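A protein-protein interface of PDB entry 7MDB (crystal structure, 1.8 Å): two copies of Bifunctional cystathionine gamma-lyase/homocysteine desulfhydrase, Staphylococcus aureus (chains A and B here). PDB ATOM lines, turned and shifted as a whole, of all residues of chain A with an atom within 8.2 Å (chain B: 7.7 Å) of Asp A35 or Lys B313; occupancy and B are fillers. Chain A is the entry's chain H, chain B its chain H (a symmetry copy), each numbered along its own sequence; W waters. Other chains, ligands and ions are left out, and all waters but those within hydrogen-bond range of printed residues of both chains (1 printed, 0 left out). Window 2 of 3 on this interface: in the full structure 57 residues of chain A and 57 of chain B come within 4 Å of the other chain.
The side-chain carboxylate of Asp A35 lies within salt-bridge range of the side-chain amino group of Lys B313. O of Leu B320 sits at hydrogen-bond distance from N of Gln A33, 3.0 Å away.
O of Ile B312 is in hydrogen-bond range of OG1 of Thr B315. OD1 of Asp A34 lies within salt-bridge range of NH2 of Arg A40, 2.9 Å away. OE1 of Gln A33 sits at hydrogen-bond distance from N of Gly A37, at 2.9 Å.
Among the printed residues, merely in contact across the chains: Leu A32 with Leu B320 (3.7 Å), Asp A34 with Lys B313 (3.6 Å), Asp A35 with Leu B320 (3.8 Å), Ile A36 with Ile B312 (3.9 Å), Ile A36 with Leu B320 (3.7 Å) and Ile A36 with Met B337 (3.7 Å).
Printed residues of chain B within 4 Å of Leu A32: Leu B320 (3.7 Å). Of the printed residues of chain B, Asp A34 touches Lys B313 (3.6 Å). Of chain B, only Lys B313 (3.1 Å) and Leu B320 (3.8 Å) come within 4 Å of Asp A35. Lys B313 touches just these residues of chain A: Asp A34 (3.6 Å) and Asp A35 (3.1 Å). No residue of chain A comes within 4 Å of Ala B314. Thr B379 touches none of the printed residues of chain A. The nearest residue of chain B that does not touch Asp A35 is Lys B309 (6.7 Å). The nearest printed residue of chain A that does not touch Ile B312 is Gln A33 (6.6 Å).
Of the 18 printed residues of chain B, 4 touch a printed residue of chain A. Hydrophobic or aromatic side chains of chain B within 4 Å of the printed part of chain A: Ile B312, Leu B320 and Met B337. Of the 9 printed residues of chain A, 5 touch a printed residue of chain B. Printed residues of chain A that touch a printed residue of chain B: Leu A32, Gln A33, Asp A34, Asp A35 and Ile A36. Hydrophobic or aromatic side chains of chain A within 4 Å of the printed part of chain B: Ile A36. Among the printed residues, 8 pairs touch across the chains. Among the printed residues, Asp or Glu carboxylates within 4 Å of a Lys or Arg side-chain nitrogen of the other chain: Asp A35 with Lys B313 (3.1 Å).
No position is printed for both chains. Of the 8 pairs that touch across the chains among the printed residues, none has its exchanged pair printed and touching as well.
Water W1 lies within hydrogen-bond range of O of Asp A34 (3.2 Å) and NZ of Lys B313 (3.2 Å).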
ATOM      1  N   LEU A  32     -26.331 -16.277 -33.367  1.00  0.00           N
ATOM      2  CA  LEU A  32     -25.972 -16.763 -32.041  1.00  0.00           C
ATOM      3  C   LEU A  32     -24.725 -16.052 -31.533  1.00  0.00           C
ATOM      4  O   LEU A  32     -23.769 -15.840 -32.285  1.00  0.00           O
ATOM      5  CB  LEU A  32     -25.725 -18.275 -32.083  1.00  0.00           C
ATOM      6  CG  LEU A  32     -26.787 -19.172 -32.723  1.00  0.00           C
ATOM      7  CD1 LEU A  32     -26.172 -20.324 -33.518  1.00  0.00           C
ATOM      8  CD2 LEU A  32     -27.672 -19.735 -31.658  1.00  0.00           C
ATOM      9  N   GLN A  33     -24.737 -15.678 -30.255  1.00  0.00           N
ATOM     10  CA  GLN A  33     -23.553 -15.172 -29.571  1.00  0.00           C
ATOM     11  C   GLN A  33     -23.105 -16.228 -28.566  1.00  0.00           C
ATOM     12  O   GLN A  33     -23.923 -16.752 -27.801  1.00  0.00           O
ATOM     13  CB  GLN A  33     -23.842 -13.838 -28.873  1.00  0.00           C
ATOM     14  CG  GLN A  33     -24.307 -12.738 -29.842  1.00  0.00           C
ATOM     15  CD  GLN A  33     -24.550 -11.405 -29.169  1.00  0.00           C
ATOM     16  OE1 GLN A  33     -23.916 -11.078 -28.165  1.00  0.00           O
ATOM     17  NE2 GLN A  33     -25.464 -10.616 -29.729  1.00  0.00           N
ATOM     18  N   ASP A  34     -21.819 -16.573 -28.593  1.00  0.00           N
ATOM     19  CA  ASP A  34     -21.340 -17.619 -27.689  1.00  0.00           C
ATOM     20  C   ASP A  34     -21.241 -17.110 -26.259  1.00  0.00           C
ATOM     21  O   ASP A  34     -21.486 -17.860 -25.308  1.00  0.00           O
ATOM     22  CB  ASP A  34     -19.997 -18.147 -28.182  1.00  0.00           C
ATOM     23  CG  ASP A  34     -20.133 -18.930 -29.473  1.00  0.00           C
ATOM     24  OD1 ASP A  34     -21.106 -19.706 -29.580  1.00  0.00           O
ATOM     25  OD2 ASP A  34     -19.291 -18.758 -30.378  1.00  0.00           O
ATOM     26  N   ASP A  35     -20.882 -15.847 -26.097  1.00  0.00           N
ATOM     27  CA  ASP A  35     -20.979 -15.125 -24.842  1.00  0.00           C
ATOM     28  C   ASP A  35     -21.541 -13.760 -25.179  1.00  0.00           C
ATOM     29  O   ASP A  35     -21.463 -13.322 -26.328  1.00  0.00           O
ATOM     30  CB  ASP A  35     -19.617 -14.986 -24.150  1.00  0.00           C
ATOM     31  CG  ASP A  35     -19.047 -16.320 -23.721  1.00  0.00           C
ATOM     32  OD1 ASP A  35     -19.435 -16.804 -22.637  1.00  0.00           O
ATOM     33  OD2 ASP A  35     -18.227 -16.889 -24.478  1.00  0.00           O
ATOM     34  N   ILE A  36     -22.103 -13.084 -24.177  1.00  0.00           N
ATOM     35  CA  ILE A  36     -22.677 -11.767 -24.432  1.00  0.00           C
ATOM     36  C   ILE A  36     -21.613 -10.871 -25.045  1.00  0.00           C
ATOM     37  O   ILE A  36     -20.570 -10.612 -24.435  1.00  0.00           O
ATOM     38  CB  ILE A  36     -23.246 -11.158 -23.151  1.00  0.00           C
ATOM     39  CG1 ILE A  36     -24.469 -11.943 -22.688  1.00  0.00           C
ATOM     40  CG2 ILE A  36     -23.613  -9.696 -23.387  1.00  0.00           C
ATOM     41  CD1 ILE A  36     -25.152 -11.345 -21.482  1.00  0.00           C
ATOM     42  N   GLY A  37     -21.866 -10.413 -26.275  1.00  0.00           N
ATOM     43  CA  GLY A  37     -20.972  -9.513 -26.967  1.00  0.00           C
ATOM     44  C   GLY A  37     -19.885 -10.171 -27.789  1.00  0.00           C
ATOM     45  O   GLY A  37     -19.162  -9.466 -28.504  1.00  0.00           O
ATOM     46  N   ASP A  38     -19.725 -11.487 -27.711  1.00  0.00           N
ATOM     47  CA  ASP A  38     -18.720 -12.199 -28.493  1.00  0.00           C
ATOM     48  C   ASP A  38     -19.391 -12.738 -29.749  1.00  0.00           C
ATOM     49  O   ASP A  38     -20.154 -13.710 -29.687  1.00  0.00           O
ATOM     50  CB  ASP A  38     -18.080 -13.324 -27.681  1.00  0.00           C
ATOM     51  CG  ASP A  38     -16.969 -14.042 -28.442  1.00  0.00           C
ATOM     52  OD1 ASP A  38     -16.500 -13.521 -29.479  1.00  0.00           O
ATOM     53  OD2 ASP A  38     -16.561 -15.134 -27.993  1.00  0.00           O
ATOM     54  N   LEU A  39     -19.106 -12.105 -30.881  1.00  0.00           N
ATOM     55  CA  LEU A  39     -19.662 -12.487 -32.172  1.00  0.00           C
ATOM     56  C   LEU A  39     -18.684 -13.410 -32.883  1.00  0.00           C
ATOM     57  O   LEU A  39     -17.502 -13.083 -33.008  1.00  0.00           O
ATOM     58  CB  LEU A  39     -19.940 -11.247 -33.025  1.00  0.00           C
ATOM     59  CG  LEU A  39     -20.600 -10.078 -32.290  1.00  0.00           C
ATOM     60  CD1 LEU A  39     -20.785  -8.845 -33.192  1.00  0.00           C
ATOM     61  CD2 LEU A  39     -21.934 -10.520 -31.699  1.00  0.00           C
ATOM     62  N   ARG A  40     -19.186 -14.553 -33.358  1.00  0.00           N
ATOM     63  CA  ARG A  40     -18.336 -15.566 -33.980  1.00  0.00           C
ATOM     64  C   ARG A  40     -17.544 -15.005 -35.153  1.00  0.00           C
ATOM     65  O   ARG A  40     -16.345 -15.270 -35.291  1.00  0.00           O
ATOM     66  CB  ARG A  40     -19.190 -16.737 -34.475  1.00  0.00           C
ATOM     67  CG  ARG A  40     -20.066 -17.353 -33.448  1.00  0.00           C
ATOM     68  CD  ARG A  40     -20.462 -18.744 -33.887  1.00  0.00           C
ATOM     69  NE  ARG A  40     -20.990 -19.489 -32.759  1.00  0.00           N
ATOM     70  CZ  ARG A  40     -21.824 -20.510 -32.870  1.00  0.00           C
ATOM     71  NH1 ARG A  40     -22.225 -20.907 -34.070  1.00  0.00           N
ATOM     72  NH2 ARG A  40     -22.251 -21.132 -31.782  1.00  0.00           N
ATOM     73  N   GLU B 306     -23.788 -11.291 -12.907  1.00  0.00           N
ATOM     74  CA  GLU B 306     -23.274 -12.654 -12.848  1.00  0.00           C
ATOM     75  C   GLU B 306     -24.412 -13.661 -12.882  1.00  0.00           C
ATOM     76  O   GLU B 306     -24.333 -14.677 -13.583  1.00  0.00           O
ATOM     77  CB  GLU B 306     -22.421 -12.836 -11.591  1.00  0.00           C
ATOM     78  CG  GLU B 306     -21.088 -12.088 -11.622  1.00  0.00           C
ATOM     79  CD  GLU B 306     -21.251 -10.564 -11.671  1.00  0.00           C
ATOM     80  OE1 GLU B 306     -22.091 -10.010 -10.910  1.00  0.00           O
ATOM     81  OE2 GLU B 306     -20.542  -9.922 -12.486  1.00  0.00           O
ATOM     82  N   SER B 307     -25.489 -13.387 -12.138  1.00  0.00           N
ATOM     83  CA  SER B 307     -26.649 -14.267 -12.182  1.00  0.00           C
ATOM     84  C   SER B 307     -27.273 -14.301 -13.571  1.00  0.00           C
ATOM     85  O   SER B 307     -27.675 -15.369 -14.044  1.00  0.00           O
ATOM     86  CB  SER B 307     -27.682 -13.847 -11.140  1.00  0.00           C
ATOM     87  OG  SER B 307     -27.098 -13.805  -9.852  1.00  0.00           O
ATOM     88  N   ALA B 308     -27.357 -13.150 -14.245  1.00  0.00           N
ATOM     89  CA  ALA B 308     -27.934 -13.125 -15.587  1.00  0.00           C
ATOM     90  C   ALA B 308     -27.120 -13.980 -16.551  1.00  0.00           C
ATOM     91  O   ALA B 308     -27.674 -14.787 -17.317  1.00  0.00           O
ATOM     92  CB  ALA B 308     -28.032 -11.683 -16.086  1.00  0.00           C
ATOM     93  N   LYS B 309     -25.792 -13.816 -16.524  1.00  0.00           N
ATOM     94  CA  LYS B 309     -24.942 -14.617 -17.396  1.00  0.00           C
ATOM     95  C   LYS B 309     -25.069 -16.101 -17.069  1.00  0.00           C
ATOM     96  O   LYS B 309     -25.163 -16.941 -17.976  1.00  0.00           O
ATOM     97  CB  LYS B 309     -23.489 -14.160 -17.279  1.00  0.00           C
ATOM     98  CG  LYS B 309     -23.190 -12.860 -18.009  1.00  0.00           C
ATOM     99  CD  LYS B 309     -21.706 -12.535 -17.964  1.00  0.00           C
ATOM    100  CE  LYS B 309     -21.431 -11.130 -18.461  1.00  0.00           C
ATOM    101  NZ  LYS B 309     -19.973 -10.871 -18.599  1.00  0.00           N
ATOM    102  N   GLN B 310     -25.091 -16.438 -15.776  1.00  0.00           N
ATOM    103  CA  GLN B 310     -25.223 -17.834 -15.369  1.00  0.00           C
ATOM    104  C   GLN B 310     -26.545 -18.422 -15.844  1.00  0.00           C
ATOM    105  O   GLN B 310     -26.591 -19.553 -16.339  1.00  0.00           O
ATOM    106  CB  GLN B 310     -25.095 -17.941 -13.847  1.00  0.00           C
ATOM    107  CG  GLN B 310     -25.063 -19.365 -13.306  1.00  0.00           C
ATOM    108  CD  GLN B 310     -24.684 -19.421 -11.834  1.00  0.00           C
ATOM    109  OE1 GLN B 310     -23.781 -18.711 -11.387  1.00  0.00           O
ATOM    110  NE2 GLN B 310     -25.375 -20.266 -11.074  1.00  0.00           N
ATOM    111  N   LEU B 311     -27.630 -17.664 -15.689  1.00  0.00           N
ATOM    112  CA  LEU B 311     -28.942 -18.073 -16.177  1.00  0.00           C
ATOM    113  C   LEU B 311     -28.887 -18.420 -17.658  1.00  0.00           C
ATOM    114  O   LEU B 311     -29.356 -19.482 -18.084  1.00  0.00           O
ATOM    115  CB  LEU B 311     -29.936 -16.937 -15.933  1.00  0.00           C
ATOM    116  CG  LEU B 311     -31.368 -17.159 -16.394  1.00  0.00           C
ATOM    117  CD1 LEU B 311     -31.966 -18.322 -15.618  1.00  0.00           C
ATOM    118  CD2 LEU B 311     -32.192 -15.896 -16.195  1.00  0.00           C
ATOM    119  N   ILE B 312     -28.310 -17.521 -18.458  1.00  0.00           N
ATOM    120  CA  ILE B 312     -28.218 -17.763 -19.895  1.00  0.00           C
ATOM    121  C   ILE B 312     -27.436 -19.044 -20.169  1.00  0.00           C
ATOM    122  O   ILE B 312     -27.852 -19.885 -20.976  1.00  0.00           O
ATOM    123  CB  ILE B 312     -27.587 -16.551 -20.600  1.00  0.00           C
ATOM    124  CG1 ILE B 312     -28.546 -15.368 -20.560  1.00  0.00           C
ATOM    125  CG2 ILE B 312     -27.209 -16.896 -22.035  1.00  0.00           C
ATOM    126  CD1 ILE B 312     -27.878 -14.046 -20.893  1.00  0.00           C
ATOM    127  N   LYS B 313     -26.305 -19.222 -19.487  1.00  0.00           N
ATOM    128  CA  LYS B 313     -25.491 -20.411 -19.737  1.00  0.00           C
ATOM    129  C   LYS B 313     -26.204 -21.693 -19.318  1.00  0.00           C
ATOM    130  O   LYS B 313     -25.987 -22.747 -19.927  1.00  0.00           O
ATOM    131  CB  LYS B 313     -24.147 -20.294 -19.019  1.00  0.00           C
ATOM    132  CG  LYS B 313     -23.336 -19.078 -19.434  1.00  0.00           C
ATOM    133  CD  LYS B 313     -21.869 -19.418 -19.682  1.00  0.00           C
ATOM    134  CE  LYS B 313     -21.286 -18.592 -20.833  1.00  0.00           C
ATOM    135  NZ  LYS B 313     -21.009 -19.394 -22.066  1.00  0.00           N
ATOM    136  N   ALA B 314     -27.076 -21.623 -18.313  1.00  0.00           N
ATOM    137  CA  ALA B 314     -27.701 -22.821 -17.766  1.00  0.00           C
ATOM    138  C   ALA B 314     -28.914 -23.305 -18.560  1.00  0.00           C
ATOM    139  O   ALA B 314     -29.330 -24.455 -18.379  1.00  0.00           O
ATOM    140  CB  ALA B 314     -28.116 -22.572 -16.315  1.00  0.00           C
ATOM    141  N   THR B 315     -29.506 -22.465 -19.409  1.00  0.00           N
ATOM    142  CA  THR B 315     -30.676 -22.878 -20.175  1.00  0.00           C
ATOM    143  C   THR B 315     -30.272 -23.777 -21.339  1.00  0.00           C
ATOM    144  O   THR B 315     -29.162 -23.681 -21.874  1.00  0.00           O
ATOM    145  CB  THR B 315     -31.439 -21.666 -20.722  1.00  0.00           C
ATOM    146  OG1 THR B 315     -30.540 -20.814 -21.445  1.00  0.00           O
ATOM    147  CG2 THR B 315     -32.101 -20.891 -19.599  1.00  0.00           C
ATOM    148  N   SER B 316     -31.186 -24.663 -21.727  1.00  0.00           N
ATOM    149  CA  SER B 316     -30.996 -25.460 -22.931  1.00  0.00           C
ATOM    150  C   SER B 316     -31.730 -24.905 -24.142  1.00  0.00           C
ATOM    151  O   SER B 316     -31.242 -25.052 -25.267  1.00  0.00           O
ATOM    152  CB  SER B 316     -31.451 -26.907 -22.695  1.00  0.00           C
ATOM    153  OG  SER B 316     -30.618 -27.561 -21.749  1.00  0.00           O
ATOM    154  N   TYR B 318     -33.166 -21.597 -24.542  1.00  0.00           N
ATOM    155  CA  TYR B 318     -33.182 -20.154 -24.752  1.00  0.00           C
ATOM    156  C   TYR B 318     -31.893 -19.743 -25.442  1.00  0.00           C
ATOM    157  O   TYR B 318     -30.798 -20.055 -24.964  1.00  0.00           O
ATOM    158  CB  TYR B 318     -33.352 -19.403 -23.434  1.00  0.00           C
ATOM    159  CG  TYR B 318     -34.704 -19.625 -22.799  1.00  0.00           C
ATOM    160  CD1 TYR B 318     -34.986 -20.805 -22.120  1.00  0.00           C
ATOM    161  CD2 TYR B 318     -35.702 -18.661 -22.889  1.00  0.00           C
ATOM    162  CE1 TYR B 318     -36.219 -21.007 -21.537  1.00  0.00           C
ATOM    163  CE2 TYR B 318     -36.935 -18.855 -22.307  1.00  0.00           C
ATOM    164  CZ  TYR B 318     -37.191 -20.042 -21.642  1.00  0.00           C
ATOM    165  OH  TYR B 318     -38.420 -20.248 -21.064  1.00  0.00           O
ATOM    166  N   LEU B 320     -29.147 -17.152 -26.997  1.00  0.00           N
ATOM    167  CA  LEU B 320     -28.584 -15.817 -26.797  1.00  0.00           C
ATOM    168  C   LEU B 320     -28.356 -15.172 -28.160  1.00  0.00           C
ATOM    169  O   LEU B 320     -27.442 -15.560 -28.895  1.00  0.00           O
ATOM    170  CB  LEU B 320     -27.279 -15.893 -26.007  1.00  0.00           C
ATOM    171  CG  LEU B 320     -26.529 -14.572 -25.834  1.00  0.00           C
ATOM    172  CD1 LEU B 320     -27.379 -13.618 -25.009  1.00  0.00           C
ATOM    173  CD2 LEU B 320     -25.162 -14.806 -25.181  1.00  0.00           C
ATOM    174  N   ILE B 331     -33.003 -14.946 -25.575  1.00  0.00           N
ATOM    175  CA  ILE B 331     -32.722 -14.370 -24.263  1.00  0.00           C
ATOM    176  C   ILE B 331     -31.627 -13.331 -24.428  1.00  0.00           C
ATOM    177  O   ILE B 331     -30.745 -13.464 -25.282  1.00  0.00           O
ATOM    178  CB  ILE B 331     -32.324 -15.475 -23.247  1.00  0.00           C
ATOM    179  CG1 ILE B 331     -32.195 -14.931 -21.814  1.00  0.00           C
ATOM    180  CG2 ILE B 331     -31.058 -16.209 -23.725  1.00  0.00           C
ATOM    181  CD1 ILE B 331     -32.380 -16.008 -20.741  1.00  0.00           C
ATOM    182  N   MET B 337     -26.488  -5.265 -23.698  1.00  0.00           N
ATOM    183  CA  MET B 337     -26.606  -5.545 -25.123  1.00  0.00           C
ATOM    184  C   MET B 337     -27.253  -4.425 -25.913  1.00  0.00           C
ATOM    185  O   MET B 337     -26.794  -4.112 -27.012  1.00  0.00           O
ATOM    186  CB  MET B 337     -27.389  -6.849 -25.330  1.00  0.00           C
ATOM    187  CG  MET B 337     -26.552  -8.077 -24.983  1.00  0.00           C
ATOM    188  SD  MET B 337     -27.458  -9.633 -24.919  1.00  0.00           S
ATOM    189  CE  MET B 337     -27.901  -9.848 -26.647  1.00  0.00           C
ATOM    190  N   GLN B 375     -35.225 -24.628 -13.957  1.00  0.00           N
ATOM    191  CA  GLN B 375     -34.014 -25.303 -13.490  1.00  0.00           C
ATOM    192  C   GLN B 375     -32.800 -24.385 -13.609  1.00  0.00           C
ATOM    193  O   GLN B 375     -31.913 -24.386 -12.733  1.00  0.00           O
ATOM    194  CB  GLN B 375     -33.792 -26.620 -14.251  1.00  0.00           C
ATOM    195  CG  GLN B 375     -33.509 -26.479 -15.746  1.00  0.00           C
ATOM    196  CD  GLN B 375     -32.045 -26.180 -16.056  1.00  0.00           C
ATOM    197  OE1 GLN B 375     -31.158 -26.435 -15.237  1.00  0.00           O
ATOM    198  NE2 GLN B 375     -31.790 -25.616 -17.238  1.00  0.00           N
ATOM    199  N   ALA B 376     -32.757 -23.564 -14.668  1.00  0.00           N
ATOM    200  CA  ALA B 376     -31.645 -22.634 -14.804  1.00  0.00           C
ATOM    201  C   ALA B 376     -31.652 -21.614 -13.673  1.00  0.00           C
ATOM    202  O   ALA B 376     -30.597 -21.299 -13.109  1.00  0.00           O
ATOM    203  CB  ALA B 376     -31.690 -21.942 -16.165  1.00  0.00           C
ATOM    204  N   THR B 379     -30.281 -22.955 -10.477  1.00  0.00           N
ATOM    205  CA  THR B 379     -28.828 -22.952 -10.292  1.00  0.00           C
ATOM    206  C   THR B 379     -28.300 -21.676  -9.641  1.00  0.00           C
ATOM    207  O   THR B 379     -27.122 -21.635  -9.267  1.00  0.00           O
ATOM    208  CB  THR B 379     -28.094 -23.152 -11.614  1.00  0.00           C
ATOM    209  OG1 THR B 379     -28.093 -21.923 -12.354  1.00  0.00           O
ATOM    210  CG2 THR B 379     -28.741 -24.266 -12.427  1.00  0.00           C
HETATM  211  O   HOH W   1     -23.564 -17.589 -22.887  1.00  0.00           O
